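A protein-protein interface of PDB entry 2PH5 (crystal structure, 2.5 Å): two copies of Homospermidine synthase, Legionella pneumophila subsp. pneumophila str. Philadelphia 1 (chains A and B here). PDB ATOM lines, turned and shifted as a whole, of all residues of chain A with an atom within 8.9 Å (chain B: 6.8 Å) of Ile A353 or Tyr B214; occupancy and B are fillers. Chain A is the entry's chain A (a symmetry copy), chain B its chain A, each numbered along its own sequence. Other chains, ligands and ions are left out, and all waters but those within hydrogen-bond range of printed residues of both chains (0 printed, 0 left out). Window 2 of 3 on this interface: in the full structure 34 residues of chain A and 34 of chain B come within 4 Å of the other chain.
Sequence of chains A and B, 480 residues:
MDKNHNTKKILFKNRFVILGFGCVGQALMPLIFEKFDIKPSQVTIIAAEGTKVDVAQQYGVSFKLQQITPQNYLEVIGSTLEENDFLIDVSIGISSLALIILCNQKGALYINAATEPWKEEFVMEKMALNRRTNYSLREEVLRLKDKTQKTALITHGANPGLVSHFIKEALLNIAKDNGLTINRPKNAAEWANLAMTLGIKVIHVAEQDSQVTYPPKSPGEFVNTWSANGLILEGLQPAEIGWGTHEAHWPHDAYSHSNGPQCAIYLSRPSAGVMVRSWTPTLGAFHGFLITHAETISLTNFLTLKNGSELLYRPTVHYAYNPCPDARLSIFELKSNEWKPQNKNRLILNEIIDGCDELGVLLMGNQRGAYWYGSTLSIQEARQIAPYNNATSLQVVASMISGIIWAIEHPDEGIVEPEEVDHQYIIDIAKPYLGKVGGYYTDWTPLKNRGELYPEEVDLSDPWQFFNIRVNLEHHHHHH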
ATOM      1  N   SER A 210     -32.411 -10.465   0.333  1.00  0.00           N
ATOM      2  CA  SER A 210     -32.205 -10.255  -1.098  1.00  0.00           C
ATOM      3  C   SER A 210     -31.364 -11.370  -1.726  1.00  0.00           C
ATOM      4  O   SER A 210     -30.862 -11.219  -2.836  1.00  0.00           O
ATOM      5  CB  SER A 210     -31.520  -8.899  -1.348  1.00  0.00           C
ATOM      6  OG  SER A 210     -30.218  -8.850  -0.788  1.00  0.00           O
ATOM      7  N   GLN A 211     -31.202 -12.489  -1.031  1.00  0.00           N
ATOM      8  CA  GLN A 211     -30.406 -13.572  -1.592  1.00  0.00           C
ATOM      9  C   GLN A 211     -31.093 -14.181  -2.817  1.00  0.00           C
ATOM     10  O   GLN A 211     -32.227 -14.643  -2.726  1.00  0.00           O
ATOM     11  CB  GLN A 211     -30.137 -14.638  -0.517  1.00  0.00           C
ATOM     12  CG  GLN A 211     -29.421 -14.039   0.708  1.00  0.00           C
ATOM     13  CD  GLN A 211     -29.287 -14.998   1.876  1.00  0.00           C
ATOM     14  OE1 GLN A 211     -28.353 -15.819   1.931  1.00  0.00           O
ATOM     15  NE2 GLN A 211     -30.226 -14.905   2.825  1.00  0.00           N
ATOM     16  N   VAL A 212     -30.416 -14.132  -3.965  1.00  0.00           N
ATOM     17  CA  VAL A 212     -30.945 -14.700  -5.204  1.00  0.00           C
ATOM     18  C   VAL A 212     -30.228 -16.015  -5.474  1.00  0.00           C
ATOM     19  O   VAL A 212     -29.188 -16.291  -4.877  1.00  0.00           O
ATOM     20  CB  VAL A 212     -30.739 -13.773  -6.422  1.00  0.00           C
ATOM     21  CG1 VAL A 212     -31.618 -12.549  -6.289  1.00  0.00           C
ATOM     22  CG2 VAL A 212     -29.276 -13.389  -6.551  1.00  0.00           C
ATOM     23  N   THR A 213     -30.760 -16.811  -6.398  1.00  0.00           N
ATOM     24  CA  THR A 213     -30.177 -18.118  -6.663  1.00  0.00           C
ATOM     25  C   THR A 213     -30.109 -18.583  -8.108  1.00  0.00           C
ATOM     26  O   THR A 213     -30.655 -17.956  -9.015  1.00  0.00           O
ATOM     27  CB  THR A 213     -30.962 -19.195  -5.941  1.00  0.00           C
ATOM     28  OG1 THR A 213     -32.302 -19.184  -6.440  1.00  0.00           O
ATOM     29  CG2 THR A 213     -30.978 -18.951  -4.442  1.00  0.00           C
ATOM     30  N   TYR A 214     -29.443 -19.719  -8.290  1.00  0.00           N
ATOM     31  CA  TYR A 214     -29.298 -20.362  -9.582  1.00  0.00           C
ATOM     32  C   TYR A 214     -29.117 -21.870  -9.356  1.00  0.00           C
ATOM     33  O   TYR A 214     -28.307 -22.293  -8.535  1.00  0.00           O
ATOM     34  CB  TYR A 214     -28.091 -19.806 -10.340  1.00  0.00           C
ATOM     35  CG  TYR A 214     -27.853 -20.547 -11.633  1.00  0.00           C
ATOM     36  CD1 TYR A 214     -28.614 -20.269 -12.779  1.00  0.00           C
ATOM     37  CD2 TYR A 214     -26.943 -21.601 -11.687  1.00  0.00           C
ATOM     38  CE1 TYR A 214     -28.476 -21.039 -13.942  1.00  0.00           C
ATOM     39  CE2 TYR A 214     -26.802 -22.370 -12.835  1.00  0.00           C
ATOM     40  CZ  TYR A 214     -27.571 -22.090 -13.953  1.00  0.00           C
ATOM     41  OH  TYR A 214     -27.459 -22.900 -15.049  1.00  0.00           O
ATOM     42  N   PRO A 215     -29.882 -22.705 -10.079  1.00  0.00           N
ATOM     43  CA  PRO A 215     -30.895 -22.364 -11.088  1.00  0.00           C
ATOM     44  C   PRO A 215     -32.135 -21.716 -10.454  1.00  0.00           C
ATOM     45  O   PRO A 215     -32.296 -21.727  -9.233  1.00  0.00           O
ATOM     46  CB  PRO A 215     -31.215 -23.720 -11.704  1.00  0.00           C
ATOM     47  CG  PRO A 215     -31.160 -24.609 -10.508  1.00  0.00           C
ATOM     48  CD  PRO A 215     -29.875 -24.157  -9.826  1.00  0.00           C
ATOM     49  N   PRO A 216     -33.034 -21.157 -11.283  1.00  0.00           N
ATOM     50  CA  PRO A 216     -34.258 -20.503 -10.803  1.00  0.00           C
ATOM     51  C   PRO A 216     -35.163 -21.441 -10.003  1.00  0.00           C
ATOM     52  O   PRO A 216     -34.879 -22.631  -9.860  1.00  0.00           O
ATOM     53  CB  PRO A 216     -34.939 -20.050 -12.095  1.00  0.00           C
ATOM     54  CG  PRO A 216     -33.806 -19.907 -13.059  1.00  0.00           C
ATOM     55  CD  PRO A 216     -32.964 -21.109 -12.752  1.00  0.00           C
ATOM     56  N   ASP A 326     -37.255 -15.841  -3.937  1.00  0.00           N
ATOM     57  CA  ASP A 326     -37.744 -17.202  -4.128  1.00  0.00           C
ATOM     58  C   ASP A 326     -38.849 -17.521  -3.124  1.00  0.00           C
ATOM     59  O   ASP A 326     -39.812 -18.223  -3.451  1.00  0.00           O
ATOM     60  CB  ASP A 326     -36.606 -18.217  -3.982  1.00  0.00           C
ATOM     61  CG  ASP A 326     -35.759 -18.341  -5.240  1.00  0.00           C
ATOM     62  OD1 ASP A 326     -34.690 -18.982  -5.170  1.00  0.00           O
ATOM     63  OD2 ASP A 326     -36.161 -17.813  -6.299  1.00  0.00           O
ATOM     64  N   ILE A 348     -32.370 -23.086   0.164  1.00  0.00           N
ATOM     65  CA  ILE A 348     -31.313 -22.600  -0.696  1.00  0.00           C
ATOM     66  C   ILE A 348     -30.091 -22.197   0.103  1.00  0.00           C
ATOM     67  O   ILE A 348     -30.151 -21.363   1.006  1.00  0.00           O
ATOM     68  CB  ILE A 348     -31.783 -21.441  -1.574  1.00  0.00           C
ATOM     69  CG1 ILE A 348     -32.535 -20.405  -0.732  1.00  0.00           C
ATOM     70  CG2 ILE A 348     -32.641 -21.997  -2.686  1.00  0.00           C
ATOM     71  CD1 ILE A 348     -32.798 -19.091  -1.455  1.00  0.00           C
ATOM     72  N   LEU A 349     -28.976 -22.822  -0.251  1.00  0.00           N
ATOM     73  CA  LEU A 349     -27.704 -22.605   0.406  1.00  0.00           C
ATOM     74  C   LEU A 349     -26.625 -22.388  -0.655  1.00  0.00           C
ATOM     75  O   LEU A 349     -26.212 -21.258  -0.914  1.00  0.00           O
ATOM     76  CB  LEU A 349     -27.380 -23.830   1.254  1.00  0.00           C
ATOM     77  CG  LEU A 349     -26.220 -23.776   2.243  1.00  0.00           C
ATOM     78  CD1 LEU A 349     -26.502 -22.736   3.324  1.00  0.00           C
ATOM     79  CD2 LEU A 349     -26.046 -25.163   2.863  1.00  0.00           C
ATOM     80  N   ASN A 350     -26.178 -23.472  -1.278  1.00  0.00           N
ATOM     81  CA  ASN A 350     -25.153 -23.373  -2.307  1.00  0.00           C
ATOM     82  C   ASN A 350     -25.662 -22.735  -3.593  1.00  0.00           C
ATOM     83  O   ASN A 350     -24.897 -22.098  -4.310  1.00  0.00           O
ATOM     84  CB  ASN A 350     -24.576 -24.751  -2.622  1.00  0.00           C
ATOM     85  CG  ASN A 350     -23.922 -25.389  -1.421  1.00  0.00           C
ATOM     86  OD1 ASN A 350     -23.333 -24.696  -0.584  1.00  0.00           O
ATOM     87  ND2 ASN A 350     -24.007 -26.712  -1.330  1.00  0.00           N
ATOM     88  N   GLU A 351     -26.947 -22.892  -3.890  1.00  0.00           N
ATOM     89  CA  GLU A 351     -27.461 -22.310  -5.113  1.00  0.00           C
ATOM     90  C   GLU A 351     -27.559 -20.790  -5.125  1.00  0.00           C
ATOM     91  O   GLU A 351     -27.693 -20.193  -6.194  1.00  0.00           O
ATOM     92  CB  GLU A 351     -28.811 -22.923  -5.501  1.00  0.00           C
ATOM     93  CG  GLU A 351     -29.839 -23.009  -4.400  1.00  0.00           C
ATOM     94  CD  GLU A 351     -29.744 -24.299  -3.588  1.00  0.00           C
ATOM     95  OE1 GLU A 351     -28.852 -24.396  -2.713  1.00  0.00           O
ATOM     96  OE2 GLU A 351     -30.566 -25.215  -3.835  1.00  0.00           O
ATOM     97  N   ILE A 352     -27.474 -20.142  -3.966  1.00  0.00           N
ATOM     98  CA  ILE A 352     -27.560 -18.693  -3.998  1.00  0.00           C
ATOM     99  C   ILE A 352     -26.237 -18.125  -4.502  1.00  0.00           C
ATOM    100  O   ILE A 352     -25.164 -18.532  -4.070  1.00  0.00           O
ATOM    101  CB  ILE A 352     -27.958 -18.079  -2.614  1.00  0.00           C
ATOM    102  CG1 ILE A 352     -26.821 -17.250  -2.049  1.00  0.00           C
ATOM    103  CG2 ILE A 352     -28.352 -19.162  -1.629  1.00  0.00           C
ATOM    104  CD1 ILE A 352     -27.287 -16.359  -0.966  1.00  0.00           C
ATOM    105  N   ILE A 353     -26.321 -17.185  -5.433  1.00  0.00           N
ATOM    106  CA  ILE A 353     -25.130 -16.604  -6.033  1.00  0.00           C
ATOM    107  C   ILE A 353     -24.822 -15.165  -5.622  1.00  0.00           C
ATOM    108  O   ILE A 353     -23.688 -14.714  -5.751  1.00  0.00           O
ATOM    109  CB  ILE A 353     -25.246 -16.660  -7.561  1.00  0.00           C
ATOM    110  CG1 ILE A 353     -26.330 -15.682  -8.036  1.00  0.00           C
ATOM    111  CG2 ILE A 353     -25.568 -18.083  -7.987  1.00  0.00           C
ATOM    112  CD1 ILE A 353     -26.693 -15.776  -9.509  1.00  0.00           C
ATOM    113  N   ASP A 354     -25.819 -14.445  -5.123  1.00  0.00           N
ATOM    114  CA  ASP A 354     -25.609 -13.056  -4.745  1.00  0.00           C
ATOM    115  C   ASP A 354     -26.652 -12.646  -3.713  1.00  0.00           C
ATOM    116  O   ASP A 354     -27.582 -13.405  -3.417  1.00  0.00           O
ATOM    117  CB  ASP A 354     -25.743 -12.173  -5.992  1.00  0.00           C
ATOM    118  CG  ASP A 354     -25.198 -10.774  -5.791  1.00  0.00           C
ATOM    119  OD1 ASP A 354     -25.729  -9.845  -6.434  1.00  0.00           O
ATOM    120  OD2 ASP A 354     -24.238 -10.587  -5.011  1.00  0.00           O
ATOM    121  N   GLY A 355     -26.489 -11.452  -3.154  1.00  0.00           N
ATOM    122  CA  GLY A 355     -27.458 -10.963  -2.188  1.00  0.00           C
ATOM    123  C   GLY A 355     -27.037 -10.927  -0.733  1.00  0.00           C
ATOM    124  O   GLY A 355     -25.943 -11.352  -0.367  1.00  0.00           O
ATOM    125  N   CYS A 356     -27.928 -10.419   0.106  1.00  0.00           N
ATOM    126  CA  CYS A 356     -27.634 -10.317   1.518  1.00  0.00           C
ATOM    127  C   CYS A 356     -28.907 -10.324   2.353  1.00  0.00           C
ATOM    128  O   CYS A 356     -30.018 -10.237   1.826  1.00  0.00           O
ATOM    129  CB  CYS A 356     -26.835  -9.043   1.789  1.00  0.00           C
ATOM    130  SG  CYS A 356     -27.718  -7.538   1.396  1.00  0.00           S
ATOM    131  N   SER A 378     -23.922 -10.181   3.736  1.00  0.00           N
ATOM    132  CA  SER A 378     -24.054 -10.676   2.377  1.00  0.00           C
ATOM    133  C   SER A 378     -23.634 -12.130   2.376  1.00  0.00           C
ATOM    134  O   SER A 378     -22.946 -12.589   3.296  1.00  0.00           O
ATOM    135  CB  SER A 378     -23.148  -9.906   1.428  1.00  0.00           C
ATOM    136  OG  SER A 378     -21.788 -10.192   1.709  1.00  0.00           O
ATOM    137  N   ILE A 379     -24.041 -12.847   1.334  1.00  0.00           N
ATOM    138  CA  ILE A 379     -23.710 -14.254   1.198  1.00  0.00           C
ATOM    139  C   ILE A 379     -22.191 -14.431   1.033  1.00  0.00           C
ATOM    140  O   ILE A 379     -21.615 -15.410   1.517  1.00  0.00           O
ATOM    141  CB  ILE A 379     -24.456 -14.886  -0.014  1.00  0.00           C
ATOM    142  CG1 ILE A 379     -24.137 -16.383  -0.103  1.00  0.00           C
ATOM    143  CG2 ILE A 379     -24.081 -14.167  -1.314  1.00  0.00           C
ATOM    144  CD1 ILE A 379     -24.650 -17.172   1.078  1.00  0.00           C
ATOM    145  N   GLN A 380     -21.543 -13.474   0.370  1.00  0.00           N
ATOM    146  CA  GLN A 380     -20.099 -13.542   0.156  1.00  0.00           C
ATOM    147  C   GLN A 380     -19.327 -13.501   1.473  1.00  0.00           C
ATOM    148  O   GLN A 380     -18.452 -14.336   1.723  1.00  0.00           O
ATOM    149  CB  GLN A 380     -19.633 -12.407  -0.767  1.00  0.00           C
ATOM    150  CG  GLN A 380     -20.067 -12.571  -2.229  1.00  0.00           C
ATOM    151  CD  GLN A 380     -21.414 -11.911  -2.540  1.00  0.00           C
ATOM    152  OE1 GLN A 380     -22.256 -11.735  -1.660  1.00  0.00           O
ATOM    153  NE2 GLN A 380     -21.620 -11.558  -3.802  1.00  0.00           N
ATOM    154  N   ARG A 383     -19.823 -16.669   3.529  1.00  0.00           N
ATOM    155  CA  ARG A 383     -19.108 -17.846   3.059  1.00  0.00           C
ATOM    156  C   ARG A 383     -17.635 -17.828   3.424  1.00  0.00           C
ATOM    157  O   ARG A 383     -17.018 -18.879   3.585  1.00  0.00           O
ATOM    158  CB  ARG A 383     -19.270 -18.002   1.548  1.00  0.00           C
ATOM    159  CG  ARG A 383     -20.560 -18.686   1.167  1.00  0.00           C
ATOM    160  CD  ARG A 383     -20.848 -18.608  -0.317  1.00  0.00           C
ATOM    161  NE  ARG A 383     -22.088 -19.311  -0.633  1.00  0.00           N
ATOM    162  CZ  ARG A 383     -22.792 -19.145  -1.747  1.00  0.00           C
ATOM    163  NH1 ARG A 383     -22.383 -18.286  -2.674  1.00  0.00           N
ATOM    164  NH2 ARG A 383     -23.908 -19.840  -1.932  1.00  0.00           N
ATOM    165  N   VAL B 212     -38.111 -18.597 -16.954  1.00  0.00           N
ATOM    166  CA  VAL B 212     -37.200 -18.180 -15.890  1.00  0.00           C
ATOM    167  C   VAL B 212     -35.924 -17.649 -16.529  1.00  0.00           C
ATOM    168  O   VAL B 212     -35.681 -17.880 -17.713  1.00  0.00           O
ATOM    169  CB  VAL B 212     -36.823 -19.336 -14.937  1.00  0.00           C
ATOM    170  CG1 VAL B 212     -38.029 -19.738 -14.118  1.00  0.00           C
ATOM    171  CG2 VAL B 212     -36.276 -20.512 -15.727  1.00  0.00           C
ATOM    172  N   THR B 213     -35.094 -16.972 -15.743  1.00  0.00           N
ATOM    173  CA  THR B 213     -33.889 -16.370 -16.295  1.00  0.00           C
ATOM    174  C   THR B 213     -32.621 -16.432 -15.459  1.00  0.00           C
ATOM    175  O   THR B 213     -32.629 -16.839 -14.299  1.00  0.00           O
ATOM    176  CB  THR B 213     -34.116 -14.893 -16.554  1.00  0.00           C
ATOM    177  OG1 THR B 213     -34.413 -14.259 -15.307  1.00  0.00           O
ATOM    178  CG2 THR B 213     -35.269 -14.677 -17.519  1.00  0.00           C
ATOM    179  N   TYR B 214     -31.531 -15.986 -16.079  1.00  0.00           N
ATOM    180  CA  TYR B 214     -30.226 -15.914 -15.450  1.00  0.00           C
ATOM    181  C   TYR B 214     -29.423 -14.795 -16.127  1.00  0.00           C
ATOM    182  O   TYR B 214     -29.350 -14.719 -17.350  1.00  0.00           O
ATOM    183  CB  TYR B 214     -29.478 -17.242 -15.586  1.00  0.00           C
ATOM    184  CG  TYR B 214     -28.072 -17.150 -15.044  1.00  0.00           C
ATOM    185  CD1 TYR B 214     -27.820 -17.226 -13.666  1.00  0.00           C
ATOM    186  CD2 TYR B 214     -27.002 -16.875 -15.894  1.00  0.00           C
ATOM    187  CE1 TYR B 214     -26.531 -17.018 -13.155  1.00  0.00           C
ATOM    188  CE2 TYR B 214     -25.724 -16.666 -15.395  1.00  0.00           C
ATOM    189  CZ  TYR B 214     -25.495 -16.732 -14.031  1.00  0.00           C
ATOM    190  OH  TYR B 214     -24.240 -16.461 -13.559  1.00  0.00           O
ATOM    191  N   PRO B 215     -28.812 -13.900 -15.333  1.00  0.00           N
ATOM    192  CA  PRO B 215     -28.805 -13.843 -13.864  1.00  0.00           C
ATOM    193  C   PRO B 215     -30.182 -13.461 -13.302  1.00  0.00           C
ATOM    194  O   PRO B 215     -31.069 -13.036 -14.044  1.00  0.00           O
ATOM    195  CB  PRO B 215     -27.758 -12.774 -13.580  1.00  0.00           C
ATOM    196  CG  PRO B 215     -28.020 -11.803 -14.682  1.00  0.00           C
ATOM    197  CD  PRO B 215     -28.139 -12.715 -15.897  1.00  0.00           C
ATOM    198  N   PRO B 216     -30.369 -13.591 -11.977  1.00  0.00           N
ATOM    199  CA  PRO B 216     -31.639 -13.263 -11.317  1.00  0.00           C
ATOM    200  C   PRO B 216     -32.055 -11.804 -11.514  1.00  0.00           C
ATOM    201  O   PRO B 216     -31.330 -11.011 -12.117  1.00  0.00           O
ATOM    202  CB  PRO B 216     -31.353 -13.560  -9.845  1.00  0.00           C
ATOM    203  CG  PRO B 216     -30.262 -14.580  -9.898  1.00  0.00           C
ATOM    204  CD  PRO B 216     -29.380 -14.056 -10.992  1.00  0.00           C
ATOM    205  N   ASP B 326     -40.330 -13.318 -12.842  1.00  0.00           N
ATOM    206  CA  ASP B 326     -39.643 -12.034 -12.741  1.00  0.00           C
ATOM    207  C   ASP B 326     -40.647 -10.885 -12.782  1.00  0.00           C
ATOM    208  O   ASP B 326     -40.471  -9.872 -12.095  1.00  0.00           O
ATOM    209  CB  ASP B 326     -38.624 -11.870 -13.873  1.00  0.00           C
ATOM    210  CG  ASP B 326     -37.315 -12.595 -13.600  1.00  0.00           C
ATOM    211  OD1 ASP B 326     -36.494 -12.701 -14.535  1.00  0.00           O
ATOM    212  OD2 ASP B 326     -37.098 -13.050 -12.457  1.00  0.00           O
ATOM    213  N   ARG B 346     -36.610  -3.735 -18.146  1.00  0.00           N
ATOM    214  CA  ARG B 346     -35.773  -4.672 -18.865  1.00  0.00           C
ATOM    215  C   ARG B 346     -36.615  -5.754 -19.512  1.00  0.00           C
ATOM    216  O   ARG B 346     -37.572  -6.239 -18.912  1.00  0.00           O
ATOM    217  CB  ARG B 346     -34.737  -5.297 -17.923  1.00  0.00           C
ATOM    218  CG  ARG B 346     -33.777  -6.257 -18.616  1.00  0.00           C
ATOM    219  CD  ARG B 346     -32.515  -6.484 -17.802  1.00  0.00           C
ATOM    220  NE  ARG B 346     -32.804  -7.059 -16.487  1.00  0.00           N
ATOM    221  CZ  ARG B 346     -32.783  -8.359 -16.209  1.00  0.00           C
ATOM    222  NH1 ARG B 346     -33.063  -8.775 -14.982  1.00  0.00           N
ATOM    223  NH2 ARG B 346     -32.469  -9.239 -17.154  1.00  0.00           N
ATOM    224  N   ASN B 350     -32.538 -13.124 -24.123  1.00  0.00           N
ATOM    225  CA  ASN B 350     -31.429 -14.064 -24.070  1.00  0.00           C
ATOM    226  C   ASN B 350     -31.173 -14.601 -22.668  1.00  0.00           C
ATOM    227  O   ASN B 350     -30.704 -15.726 -22.515  1.00  0.00           O
ATOM    228  CB  ASN B 350     -30.153 -13.416 -24.602  1.00  0.00           C
ATOM    229  CG  ASN B 350     -30.284 -12.985 -26.042  1.00  0.00           C
ATOM    230  OD1 ASN B 350     -30.970 -13.638 -26.835  1.00  0.00           O
ATOM    231  ND2 ASN B 350     -29.620 -11.889 -26.397  1.00  0.00           N
ATOM    232  N   GLU B 351     -31.483 -13.816 -21.643  1.00  0.00           N
ATOM    233  CA  GLU B 351     -31.239 -14.292 -20.296  1.00  0.00           C
ATOM    234  C   GLU B 351     -32.155 -15.413 -19.820  1.00  0.00           C
ATOM    235  O   GLU B 351     -31.847 -16.079 -18.831  1.00  0.00           O
ATOM    236  CB  GLU B 351     -31.254 -13.141 -19.285  1.00  0.00           C
ATOM    237  CG  GLU B 351     -32.421 -12.189 -19.382  1.00  0.00           C
ATOM    238  CD  GLU B 351     -32.176 -11.034 -20.350  1.00  0.00           C
ATOM    239  OE1 GLU B 351     -32.290 -11.244 -21.580  1.00  0.00           O
ATOM    240  OE2 GLU B 351     -31.864  -9.917 -19.870  1.00  0.00           O
ATOM    241  N   ILE B 352     -33.266 -15.656 -20.510  1.00  0.00           N
ATOM    242  CA  ILE B 352     -34.122 -16.733 -20.049  1.00  0.00           C
ATOM    243  C   ILE B 352     -33.496 -18.069 -20.435  1.00  0.00           C
ATOM    244  O   ILE B 352     -33.050 -18.261 -21.561  1.00  0.00           O
ATOM    245  CB  ILE B 352     -35.590 -16.612 -20.580  1.00  0.00           C
ATOM    246  CG1 ILE B 352     -35.917 -17.760 -21.514  1.00  0.00           C
ATOM    247  CG2 ILE B 352     -35.808 -15.289 -21.285  1.00  0.00           C
ATOM    248  CD1 ILE B 352     -37.375 -17.893 -21.719  1.00  0.00           C
ATOM    249  N   ILE B 353     -33.455 -18.994 -19.484  1.00  0.00           N
ATOM    250  CA  ILE B 353     -32.833 -20.289 -19.713  1.00  0.00           C
ATOM    251  C   ILE B 353     -33.797 -21.469 -19.825  1.00  0.00           C
ATOM    252  O   ILE B 353     -33.442 -22.506 -20.376  1.00  0.00           O
ATOM    253  CB  ILE B 353     -31.831 -20.581 -18.589  1.00  0.00           C
ATOM    254  CG1 ILE B 353     -32.584 -20.836 -17.275  1.00  0.00           C
ATOM    255  CG2 ILE B 353     -30.873 -19.408 -18.454  1.00  0.00           C
ATOM    256  CD1 ILE B 353     -31.712 -20.943 -16.035  1.00  0.00           C
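The side-chain hydroxyl of Thr B213 is in hydrogen-bond range of the side-chain carboxylate of Asp B326 (2.7 Å).
The backbone NH of Tyr B214 sits at hydrogen-bond distance from the backbone carbonyl oxygen of Glu B351.
The backbone NH of Ile A353 lies within hydrogen-bond range of the backbone carbonyl oxygen of Val A212, 3.1 Å away.
O of Asp A354 lies within hydrogen-bond range of N of Val A212, at 3.0 Å.
The side-chain carboxylate (OD1) of Asp A326 sits at hydrogen-bond distance from the side-chain hydroxyl (OG1) of Thr A213, 2.7 Å away.
O of Glu A351 sits at hydrogen-bond distance from N of Tyr A214, 2.8 Å away.
CB of Pro B216 touches CB of Val A212, at 3.5 Å.
O of Thr A213 touches CG of Pro B216, at 3.5 Å.
Tyr B214 touches Tyr A214.
Ile B353 touches Tyr A214.
Val B212 touches Pro A216 (CB to CB, 3.5 Å).
Pro A216 touches Thr B213.
Pro A216 touches Ile B353.
Tyr B214 touches Ile A353 (CE1 to CD1, 3.9 Å).
CD1 of Ile A353 touches CD of Pro B216 (3.5 Å).
Tyr B214 touches two residues of chain A.
Of chain A, only Pro A216 (3.5 Å) comes within 4 Å of Thr B213.
Pro B215 touches none of the printed residues of chain A.
Of the printed residues of chain A, Pro B216 touches Val A212, Thr A213 and Ile A353.
Of the printed residues of chain B, Pro A216 touches Val B212, Thr B213 and Ile B353.
Hydrophobic or aromatic side chains of chain B that line the printed part of chain A: Val B212, Tyr B214, Pro B216 and Ile B353.
Among the printed residues, no Asp or Glu carboxylate lies within 4 Å of a Lys or Arg side-chain nitrogen of the other chain.
Val A212 touches Pro B216, and with the chains exchanged Pro A216 touches Val B212.
Thr A213 touches Pro B216, and with the chains exchanged Pro A216 touches Thr B213.
Tyr A214 touches its own counterpart, Tyr B214.
Pro A216 touches Ile B353, and with the chains exchanged Ile A353 touches Pro B216.
Of the 9 pairs that touch across the chains among the printed residues, 9 have their exchanged pair printed and touching as well.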
